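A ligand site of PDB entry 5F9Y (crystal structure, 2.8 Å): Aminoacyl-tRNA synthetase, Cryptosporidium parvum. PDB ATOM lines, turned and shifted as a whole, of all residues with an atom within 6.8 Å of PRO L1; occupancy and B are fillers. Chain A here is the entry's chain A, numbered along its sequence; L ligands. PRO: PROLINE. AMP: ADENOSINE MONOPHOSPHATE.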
ATOM      1  N   PRO A 122       8.177 -10.101 -27.483  1.00  0.00           N
ATOM      2  CA  PRO A 122       7.660 -10.839 -26.327  1.00  0.00           C
ATOM      3  C   PRO A 122       6.242 -10.436 -25.972  1.00  0.00           C
ATOM      4  O   PRO A 122       5.557 -11.182 -25.256  1.00  0.00           O
ATOM      5  CB  PRO A 122       8.642 -10.463 -25.209  1.00  0.00           C
ATOM      6  CG  PRO A 122       9.058  -9.068 -25.567  1.00  0.00           C
ATOM      7  CD  PRO A 122       9.044  -8.986 -27.081  1.00  0.00           C
ATOM      8  N   THR A 123       5.791  -9.285 -26.458  1.00  0.00           N
ATOM      9  CA  THR A 123       4.449  -8.763 -26.286  1.00  0.00           C
ATOM     10  C   THR A 123       4.308  -7.597 -27.257  1.00  0.00           C
ATOM     11  O   THR A 123       5.296  -7.128 -27.833  1.00  0.00           O
ATOM     12  CB  THR A 123       4.179  -8.318 -24.846  1.00  0.00           C
ATOM     13  OG1 THR A 123       2.820  -7.879 -24.718  1.00  0.00           O
ATOM     14  CG2 THR A 123       5.121  -7.196 -24.442  1.00  0.00           C
ATOM     15  N   SER A 124       3.081  -7.121 -27.443  1.00  0.00           N
ATOM     16  CA  SER A 124       2.797  -6.134 -28.472  1.00  0.00           C
ATOM     17  C   SER A 124       2.414  -4.768 -27.915  1.00  0.00           C
ATOM     18  O   SER A 124       1.856  -3.938 -28.651  1.00  0.00           O
ATOM     19  CB  SER A 124       1.692  -6.648 -29.401  1.00  0.00           C
ATOM     20  OG  SER A 124       2.091  -7.859 -30.037  1.00  0.00           O
ATOM     21  N   GLU A 125       2.691  -4.506 -26.639  1.00  0.00           N
ATOM     22  CA  GLU A 125       2.397  -3.190 -26.077  1.00  0.00           C
ATOM     23  C   GLU A 125       3.183  -2.095 -26.792  1.00  0.00           C
ATOM     24  O   GLU A 125       2.613  -1.119 -27.274  1.00  0.00           O
ATOM     25  CB  GLU A 125       2.698  -3.162 -24.570  1.00  0.00           C
ATOM     26  CG  GLU A 125       1.524  -3.543 -23.684  1.00  0.00           C
ATOM     27  CD  GLU A 125       1.310  -5.044 -23.608  1.00  0.00           C
ATOM     28  OE1 GLU A 125       2.141  -5.794 -24.147  1.00  0.00           O
ATOM     29  OE2 GLU A 125       0.307  -5.462 -22.985  1.00  0.00           O
ATOM     30  N   TYR A 129       0.736   0.402 -29.370  1.00  0.00           N
ATOM     31  CA  TYR A 129       0.336   1.643 -28.720  1.00  0.00           C
ATOM     32  C   TYR A 129       0.911   2.895 -29.388  1.00  0.00           C
ATOM     33  O   TYR A 129       0.248   3.945 -29.377  1.00  0.00           O
ATOM     34  CB  TYR A 129       0.712   1.608 -27.230  1.00  0.00           C
ATOM     35  CG  TYR A 129      -0.061   0.552 -26.449  1.00  0.00           C
ATOM     36  CD1 TYR A 129      -1.097  -0.161 -27.051  1.00  0.00           C
ATOM     37  CD2 TYR A 129       0.239   0.290 -25.125  1.00  0.00           C
ATOM     38  CE1 TYR A 129      -1.799  -1.121 -26.355  1.00  0.00           C
ATOM     39  CE2 TYR A 129      -0.473  -0.670 -24.410  1.00  0.00           C
ATOM     40  CZ  TYR A 129      -1.486  -1.375 -25.040  1.00  0.00           C
ATOM     41  OH  TYR A 129      -2.207  -2.328 -24.354  1.00  0.00           O
ATOM     42  N   ARG A 154       9.902 -16.052 -25.945  1.00  0.00           N
ATOM     43  CA  ARG A 154      10.481 -15.564 -24.700  1.00  0.00           C
ATOM     44  C   ARG A 154      11.536 -16.562 -24.269  1.00  0.00           C
ATOM     45  O   ARG A 154      11.207 -17.715 -23.935  1.00  0.00           O
ATOM     46  CB  ARG A 154       9.416 -15.384 -23.611  1.00  0.00           C
ATOM     47  CG  ARG A 154       8.455 -14.234 -23.846  1.00  0.00           C
ATOM     48  CD  ARG A 154       7.452 -14.123 -22.714  1.00  0.00           C
ATOM     49  NE  ARG A 154       6.452 -13.097 -22.958  1.00  0.00           N
ATOM     50  CZ  ARG A 154       5.431 -12.826 -22.147  1.00  0.00           C
ATOM     51  NH1 ARG A 154       5.272 -13.525 -21.028  1.00  0.00           N
ATOM     52  NH2 ARG A 154       4.563 -11.874 -22.459  1.00  0.00           N
ATOM     53  N   TRP A 171      -0.467 -17.832 -28.507  1.00  0.00           N
ATOM     54  CA  TRP A 171      -1.307 -17.133 -27.541  1.00  0.00           C
ATOM     55  C   TRP A 171      -2.284 -16.232 -28.277  1.00  0.00           C
ATOM     56  O   TRP A 171      -2.340 -16.200 -29.506  1.00  0.00           O
ATOM     57  CB  TRP A 171      -0.449 -16.349 -26.540  1.00  0.00           C
ATOM     58  CG  TRP A 171      -0.038 -14.935 -26.946  1.00  0.00           C
ATOM     59  CD1 TRP A 171       0.050 -14.413 -28.214  1.00  0.00           C
ATOM     60  CD2 TRP A 171       0.367 -13.882 -26.060  1.00  0.00           C
ATOM     61  NE1 TRP A 171       0.459 -13.099 -28.160  1.00  0.00           N
ATOM     62  CE2 TRP A 171       0.668 -12.757 -26.854  1.00  0.00           C
ATOM     63  CE3 TRP A 171       0.500 -13.782 -24.669  1.00  0.00           C
ATOM     64  CZ2 TRP A 171       1.093 -11.554 -26.300  1.00  0.00           C
ATOM     65  CZ3 TRP A 171       0.923 -12.588 -24.126  1.00  0.00           C
ATOM     66  CH2 TRP A 171       1.215 -11.488 -24.944  1.00  0.00           C
ATOM     67  N   GLN A 172      -3.055 -15.508 -27.487  1.00  0.00           N
ATOM     68  CA  GLN A 172      -3.933 -14.446 -27.945  1.00  0.00           C
ATOM     69  C   GLN A 172      -3.701 -13.246 -27.033  1.00  0.00           C
ATOM     70  O   GLN A 172      -3.522 -13.419 -25.830  1.00  0.00           O
ATOM     71  CB  GLN A 172      -5.401 -14.903 -27.905  1.00  0.00           C
ATOM     72  CG  GLN A 172      -6.442 -13.841 -27.589  1.00  0.00           C
ATOM     73  CD  GLN A 172      -6.563 -13.556 -26.108  1.00  0.00           C
ATOM     74  OE1 GLN A 172      -6.651 -14.477 -25.290  1.00  0.00           O
ATOM     75  NE2 GLN A 172      -6.561 -12.285 -25.746  1.00  0.00           N
ATOM     76  N   GLU A 173      -3.708 -12.045 -27.601  1.00  0.00           N
ATOM     77  CA  GLU A 173      -3.545 -10.824 -26.818  1.00  0.00           C
ATOM     78  C   GLU A 173      -4.559  -9.795 -27.264  1.00  0.00           C
ATOM     79  O   GLU A 173      -4.598  -9.417 -28.434  1.00  0.00           O
ATOM     80  CB  GLU A 173      -2.121 -10.270 -26.916  1.00  0.00           C
ATOM     81  CG  GLU A 173      -1.570 -10.101 -28.313  1.00  0.00           C
ATOM     82  CD  GLU A 173      -0.239  -9.382 -28.320  1.00  0.00           C
ATOM     83  OE1 GLU A 173       0.003  -8.580 -27.392  1.00  0.00           O
ATOM     84  OE2 GLU A 173       0.579  -9.624 -29.243  1.00  0.00           O
ATOM     85  N   GLY A 174      -5.398  -9.358 -26.325  1.00  0.00           N
ATOM     86  CA  GLY A 174      -6.354  -8.291 -26.582  1.00  0.00           C
ATOM     87  C   GLY A 174      -5.888  -6.997 -25.943  1.00  0.00           C
ATOM     88  O   GLY A 174      -5.341  -6.998 -24.839  1.00  0.00           O
ATOM     89  N   HIS A 175      -6.076  -5.896 -26.661  1.00  0.00           N
ATOM     90  CA  HIS A 175      -5.687  -4.572 -26.202  1.00  0.00           C
ATOM     91  C   HIS A 175      -6.838  -3.621 -26.471  1.00  0.00           C
ATOM     92  O   HIS A 175      -7.252  -3.465 -27.621  1.00  0.00           O
ATOM     93  CB  HIS A 175      -4.408  -4.106 -26.892  1.00  0.00           C
ATOM     94  CG  HIS A 175      -3.239  -5.028 -26.720  1.00  0.00           C
ATOM     95  ND1 HIS A 175      -2.202  -4.758 -25.858  1.00  0.00           N
ATOM     96  CD2 HIS A 175      -2.956  -6.211 -27.294  1.00  0.00           C
ATOM     97  CE1 HIS A 175      -1.321  -5.745 -25.904  1.00  0.00           C
ATOM     98  NE2 HIS A 175      -1.760  -6.642 -26.769  1.00  0.00           N
ATOM     99  N   TYR A 195     -11.969 -16.044 -19.472  1.00  0.00           N
ATOM    100  CA  TYR A 195     -10.822 -16.909 -19.202  1.00  0.00           C
ATOM    101  C   TYR A 195     -11.185 -18.010 -18.225  1.00  0.00           C
ATOM    102  O   TYR A 195     -10.804 -19.176 -18.410  1.00  0.00           O
ATOM    103  CB  TYR A 195      -9.655 -16.080 -18.672  1.00  0.00           C
ATOM    104  CG  TYR A 195      -8.907 -15.311 -19.747  1.00  0.00           C
ATOM    105  CD1 TYR A 195      -8.060 -14.255 -19.405  1.00  0.00           C
ATOM    106  CD2 TYR A 195      -9.048 -15.640 -21.080  1.00  0.00           C
ATOM    107  CE1 TYR A 195      -7.383 -13.553 -20.380  1.00  0.00           C
ATOM    108  CE2 TYR A 195      -8.362 -14.939 -22.065  1.00  0.00           C
ATOM    109  CZ  TYR A 195      -7.540 -13.899 -21.705  1.00  0.00           C
ATOM    110  OH  TYR A 195      -6.866 -13.205 -22.692  1.00  0.00           O
ATOM    111  N   PHE A 218       1.208  -6.833 -13.246  1.00  0.00           N
ATOM    112  CA  PHE A 218       1.929  -6.472 -14.449  1.00  0.00           C
ATOM    113  C   PHE A 218       2.823  -5.265 -14.156  1.00  0.00           C
ATOM    114  O   PHE A 218       2.390  -4.328 -13.458  1.00  0.00           O
ATOM    115  CB  PHE A 218       0.946  -6.157 -15.581  1.00  0.00           C
ATOM    116  CG  PHE A 218       1.556  -6.201 -16.956  1.00  0.00           C
ATOM    117  CD1 PHE A 218       1.916  -7.410 -17.522  1.00  0.00           C
ATOM    118  CD2 PHE A 218       1.753  -5.043 -17.677  1.00  0.00           C
ATOM    119  CE1 PHE A 218       2.462  -7.460 -18.788  1.00  0.00           C
ATOM    120  CE2 PHE A 218       2.303  -5.084 -18.942  1.00  0.00           C
ATOM    121  CZ  PHE A 218       2.662  -6.293 -19.507  1.00  0.00           C
ATOM    122  N   GLN A 239      -0.102 -20.226 -12.885  1.00  0.00           N
ATOM    123  CA  GLN A 239      -0.940 -19.109 -13.304  1.00  0.00           C
ATOM    124  C   GLN A 239      -1.582 -19.424 -14.647  1.00  0.00           C
ATOM    125  O   GLN A 239      -0.891 -19.734 -15.623  1.00  0.00           O
ATOM    126  CB  GLN A 239      -0.096 -17.837 -13.406  1.00  0.00           C
ATOM    127  CG  GLN A 239      -0.903 -16.592 -13.756  1.00  0.00           C
ATOM    128  CD  GLN A 239      -0.018 -15.410 -14.062  1.00  0.00           C
ATOM    129  OE1 GLN A 239       0.251 -14.586 -13.192  1.00  0.00           O
ATOM    130  NE2 GLN A 239       0.428 -15.314 -15.310  1.00  0.00           N
ATOM    131  N   THR A 242      -4.170 -13.998 -17.422  1.00  0.00           N
ATOM    132  CA  THR A 242      -4.115 -12.678 -16.790  1.00  0.00           C
ATOM    133  C   THR A 242      -4.888 -11.660 -17.605  1.00  0.00           C
ATOM    134  O   THR A 242      -4.959 -11.740 -18.841  1.00  0.00           O
ATOM    135  CB  THR A 242      -2.665 -12.191 -16.634  1.00  0.00           C
ATOM    136  OG1 THR A 242      -1.960 -12.371 -17.874  1.00  0.00           O
ATOM    137  CG2 THR A 242      -1.956 -12.965 -15.534  1.00  0.00           C
ATOM    138  N   SER A 243      -5.476 -10.684 -16.907  1.00  0.00           N
ATOM    139  CA  SER A 243      -6.221  -9.591 -17.508  1.00  0.00           C
ATOM    140  C   SER A 243      -5.830  -8.307 -16.792  1.00  0.00           C
ATOM    141  O   SER A 243      -6.151  -8.137 -15.604  1.00  0.00           O
ATOM    142  CB  SER A 243      -7.727  -9.842 -17.420  1.00  0.00           C
ATOM    143  OG  SER A 243      -8.454  -8.820 -18.082  1.00  0.00           O
ATOM    144  N   HIS A 244      -5.131  -7.420 -17.488  1.00  0.00           N
ATOM    145  CA  HIS A 244      -4.504  -6.250 -16.863  1.00  0.00           C
ATOM    146  C   HIS A 244      -5.327  -4.994 -17.110  1.00  0.00           C
ATOM    147  O   HIS A 244      -5.733  -4.716 -18.243  1.00  0.00           O
ATOM    148  CB  HIS A 244      -3.084  -6.041 -17.414  1.00  0.00           C
ATOM    149  CG  HIS A 244      -2.278  -7.298 -17.480  1.00  0.00           C
ATOM    150  ND1 HIS A 244      -1.783  -7.923 -16.353  1.00  0.00           N
ATOM    151  CD2 HIS A 244      -1.863  -8.038 -18.534  1.00  0.00           C
ATOM    152  CE1 HIS A 244      -1.105  -9.000 -16.711  1.00  0.00           C
ATOM    153  NE2 HIS A 244      -1.138  -9.090 -18.027  1.00  0.00           N
ATOM    154  N   SER A 272      -5.053  -4.800 -21.278  1.00  0.00           N
ATOM    155  CA  SER A 272      -4.411  -5.830 -22.085  1.00  0.00           C
ATOM    156  C   SER A 272      -4.590  -7.161 -21.388  1.00  0.00           C
ATOM    157  O   SER A 272      -4.527  -7.237 -20.154  1.00  0.00           O
ATOM    158  CB  SER A 272      -2.933  -5.526 -22.328  1.00  0.00           C
ATOM    159  OG  SER A 272      -2.166  -5.727 -21.145  1.00  0.00           O
ATOM    160  N   TRP A 273      -4.824  -8.210 -22.168  1.00  0.00           N
ATOM    161  CA  TRP A 273      -5.157  -9.520 -21.634  1.00  0.00           C
ATOM    162  C   TRP A 273      -4.671 -10.604 -22.593  1.00  0.00           C
ATOM    163  O   TRP A 273      -4.714 -10.430 -23.812  1.00  0.00           O
ATOM    164  CB  TRP A 273      -6.665  -9.656 -21.378  1.00  0.00           C
ATOM    165  CG  TRP A 273      -7.506  -8.748 -22.241  1.00  0.00           C
ATOM    166  CD1 TRP A 273      -7.752  -7.426 -22.040  1.00  0.00           C
ATOM    167  CD2 TRP A 273      -8.195  -9.122 -23.442  1.00  0.00           C
ATOM    168  NE1 TRP A 273      -8.563  -6.941 -23.043  1.00  0.00           N
ATOM    169  CE2 TRP A 273      -8.842  -7.962 -23.921  1.00  0.00           C
ATOM    170  CE3 TRP A 273      -8.334 -10.306 -24.168  1.00  0.00           C
ATOM    171  CZ2 TRP A 273      -9.618  -7.953 -25.081  1.00  0.00           C
ATOM    172  CZ3 TRP A 273      -9.101 -10.301 -25.318  1.00  0.00           C
ATOM    173  CH2 TRP A 273      -9.734  -9.131 -25.755  1.00  0.00           C
ATOM    174  N   GLY A 274      -4.216 -11.715 -22.031  1.00  0.00           N
ATOM    175  CA  GLY A 274      -3.615 -12.777 -22.822  1.00  0.00           C
ATOM    176  C   GLY A 274      -3.935 -14.144 -22.286  1.00  0.00           C
ATOM    177  O   GLY A 274      -4.111 -14.342 -21.076  1.00  0.00           O
ATOM    178  N   LEU A 275      -4.012 -15.119 -23.193  1.00  0.00           N
ATOM    179  CA  LEU A 275      -4.180 -16.526 -22.860  1.00  0.00           C
ATOM    180  C   LEU A 275      -3.327 -17.349 -23.804  1.00  0.00           C
ATOM    181  O   LEU A 275      -3.417 -17.191 -25.026  1.00  0.00           O
ATOM    182  CB  LEU A 275      -5.650 -16.949 -22.967  1.00  0.00           C
ATOM    183  CG  LEU A 275      -5.944 -18.441 -22.791  1.00  0.00           C
ATOM    184  CD1 LEU A 275      -5.626 -18.882 -21.370  1.00  0.00           C
ATOM    185  CD2 LEU A 275      -7.383 -18.753 -23.144  1.00  0.00           C
HETATM  186  N   PRO L   1       0.356  -8.302 -22.546  1.00  0.00           N
HETATM  187  CA  PRO L   1       0.013  -8.963 -21.284  1.00  0.00           C
HETATM  188  C   PRO L   1       1.089  -9.932 -20.808  1.00  0.00           C
HETATM  189  O   PRO L   1       2.165 -10.008 -21.408  1.00  0.00           O
HETATM  190  CB  PRO L   1      -1.284  -9.717 -21.615  1.00  0.00           C
HETATM  191  CG  PRO L   1      -1.274  -9.860 -23.100  1.00  0.00           C
HETATM  192  CD  PRO L   1      -0.599  -8.631 -23.616  1.00  0.00           C
HETATM  193  OXT PRO L   1       0.915 -10.639 -19.821  1.00  0.00           O
HETATM  194  P   AMP L   2       3.117 -13.242 -17.284  1.00  0.00           P
HETATM  195  O1P AMP L   2       2.701 -12.380 -16.122  1.00  0.00           O
HETATM  196  O2P AMP L   2       4.050 -12.559 -18.255  1.00  0.00           O
HETATM  197  O3P AMP L   2       3.536 -14.652 -16.917  1.00  0.00           O
HETATM  198  O5' AMP L   2       1.778 -13.440 -18.123  1.00  0.00           O
HETATM  199  C5' AMP L   2       1.824 -13.834 -19.491  1.00  0.00           C
HETATM  200  C4' AMP L   2       0.901 -15.002 -19.770  1.00  0.00           C
HETATM  201  O4' AMP L   2       1.610 -15.953 -20.614  1.00  0.00           O
HETATM  202  C3' AMP L   2       0.443 -15.790 -18.549  1.00  0.00           C
HETATM  203  O3' AMP L   2      -0.851 -16.345 -18.801  1.00  0.00           O
HETATM  204  C2' AMP L   2       1.474 -16.910 -18.459  1.00  0.00           C
HETATM  205  O2' AMP L   2       1.013 -18.070 -17.796  1.00  0.00           O
HETATM  206  C1' AMP L   2       1.766 -17.187 -19.935  1.00  0.00           C
HETATM  207  N9  AMP L   2       3.135 -17.652 -20.189  1.00  0.00           N
HETATM  208  C8  AMP L   2       4.244 -16.996 -19.796  1.00  0.00           C
HETATM  209  N7  AMP L   2       5.365 -17.672 -20.166  1.00  0.00           N
HETATM  210  C5  AMP L   2       4.969 -18.775 -20.816  1.00  0.00           C
HETATM  211  C6  AMP L   2       5.650 -19.925 -21.467  1.00  0.00           C
HETATM  212  N6  AMP L   2       6.999 -20.005 -21.494  1.00  0.00           N
HETATM  213  N1  AMP L   2       4.874 -20.875 -22.034  1.00  0.00           N
HETATM  214  C2  AMP L   2       3.525 -20.796 -22.006  1.00  0.00           C
HETATM  215  N3  AMP L   2       2.848 -19.794 -21.428  1.00  0.00           N
HETATM  216  C4  AMP L   2       3.501 -18.769 -20.822  1.00  0.00           C
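O of Trp 273 lies within hydrogen-bond range of N of Gly 174, 2.8 Å away. The guanidinium group (NH2) of Arg 154 lies within hydrogen-bond range of the backbone carbonyl oxygen (O) of Pro 122 (3.0 Å). The backbone carbonyl oxygen of Trp 273 lies close to the side-chain amide nitrogen of Gln 172, 3.3 Å away. The side-chain carboxylate of Glu 173 lies within hydrogen-bond range of a ring nitrogen (NE2) of His 175. The side-chain hydroxyl (OH) of Tyr 129 lies within hydrogen-bond range of a ring nitrogen (ND1) of His 175 (2.9 Å). OE2 of Glu 125 lies within hydrogen-bond range of OG of Ser 272. The side-chain hydroxyl (OG1) of Thr 242 is in hydrogen-bond range of a ring nitrogen (NE2) of His 244 (3.4 Å). N of Gly 274 lies close to OH of Tyr 195.
An oxygen (O2') of AMP L2 sits at hydrogen-bond distance from the backbone carbonyl oxygen of Gln 239 (3.3 Å). OG1 of Thr 123 lies within hydrogen-bond range of N of PRO L1 (3.3 Å). An oxygen (O2P) of AMP L2 lies within salt-bridge range of the guanidinium group of Arg 154, 3.2 Å away. An oxygen (O) of PRO L1 is in salt-bridge range of the guanidinium group (NH2) of Arg 154 (3.2 Å). NE2 of His 244 lies within hydrogen-bond range of OXT of PRO L1, 3.1 Å away. OE2 of Glu 125 lies within salt-bridge range of N of PRO L1 (2.9 Å).
Residues that only touch PRO L1: Trp 171 (3.5 Å), Glu 173 (3.8 Å), His 175 (3.8 Å), Phe 218 (3.5 Å), Thr 242 (3.9 Å), Ser 272 (3.9 Å), Trp 273 (3.5 Å) and Gly 274 (3.6 Å). Hydrophobic or aromatic side chains within 4 Å of PRO L1: Trp 171, His 175, Phe 218 and His 244. The nearest printed residue that does not touch PRO L1 is Gln 172 (5.0 Å).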
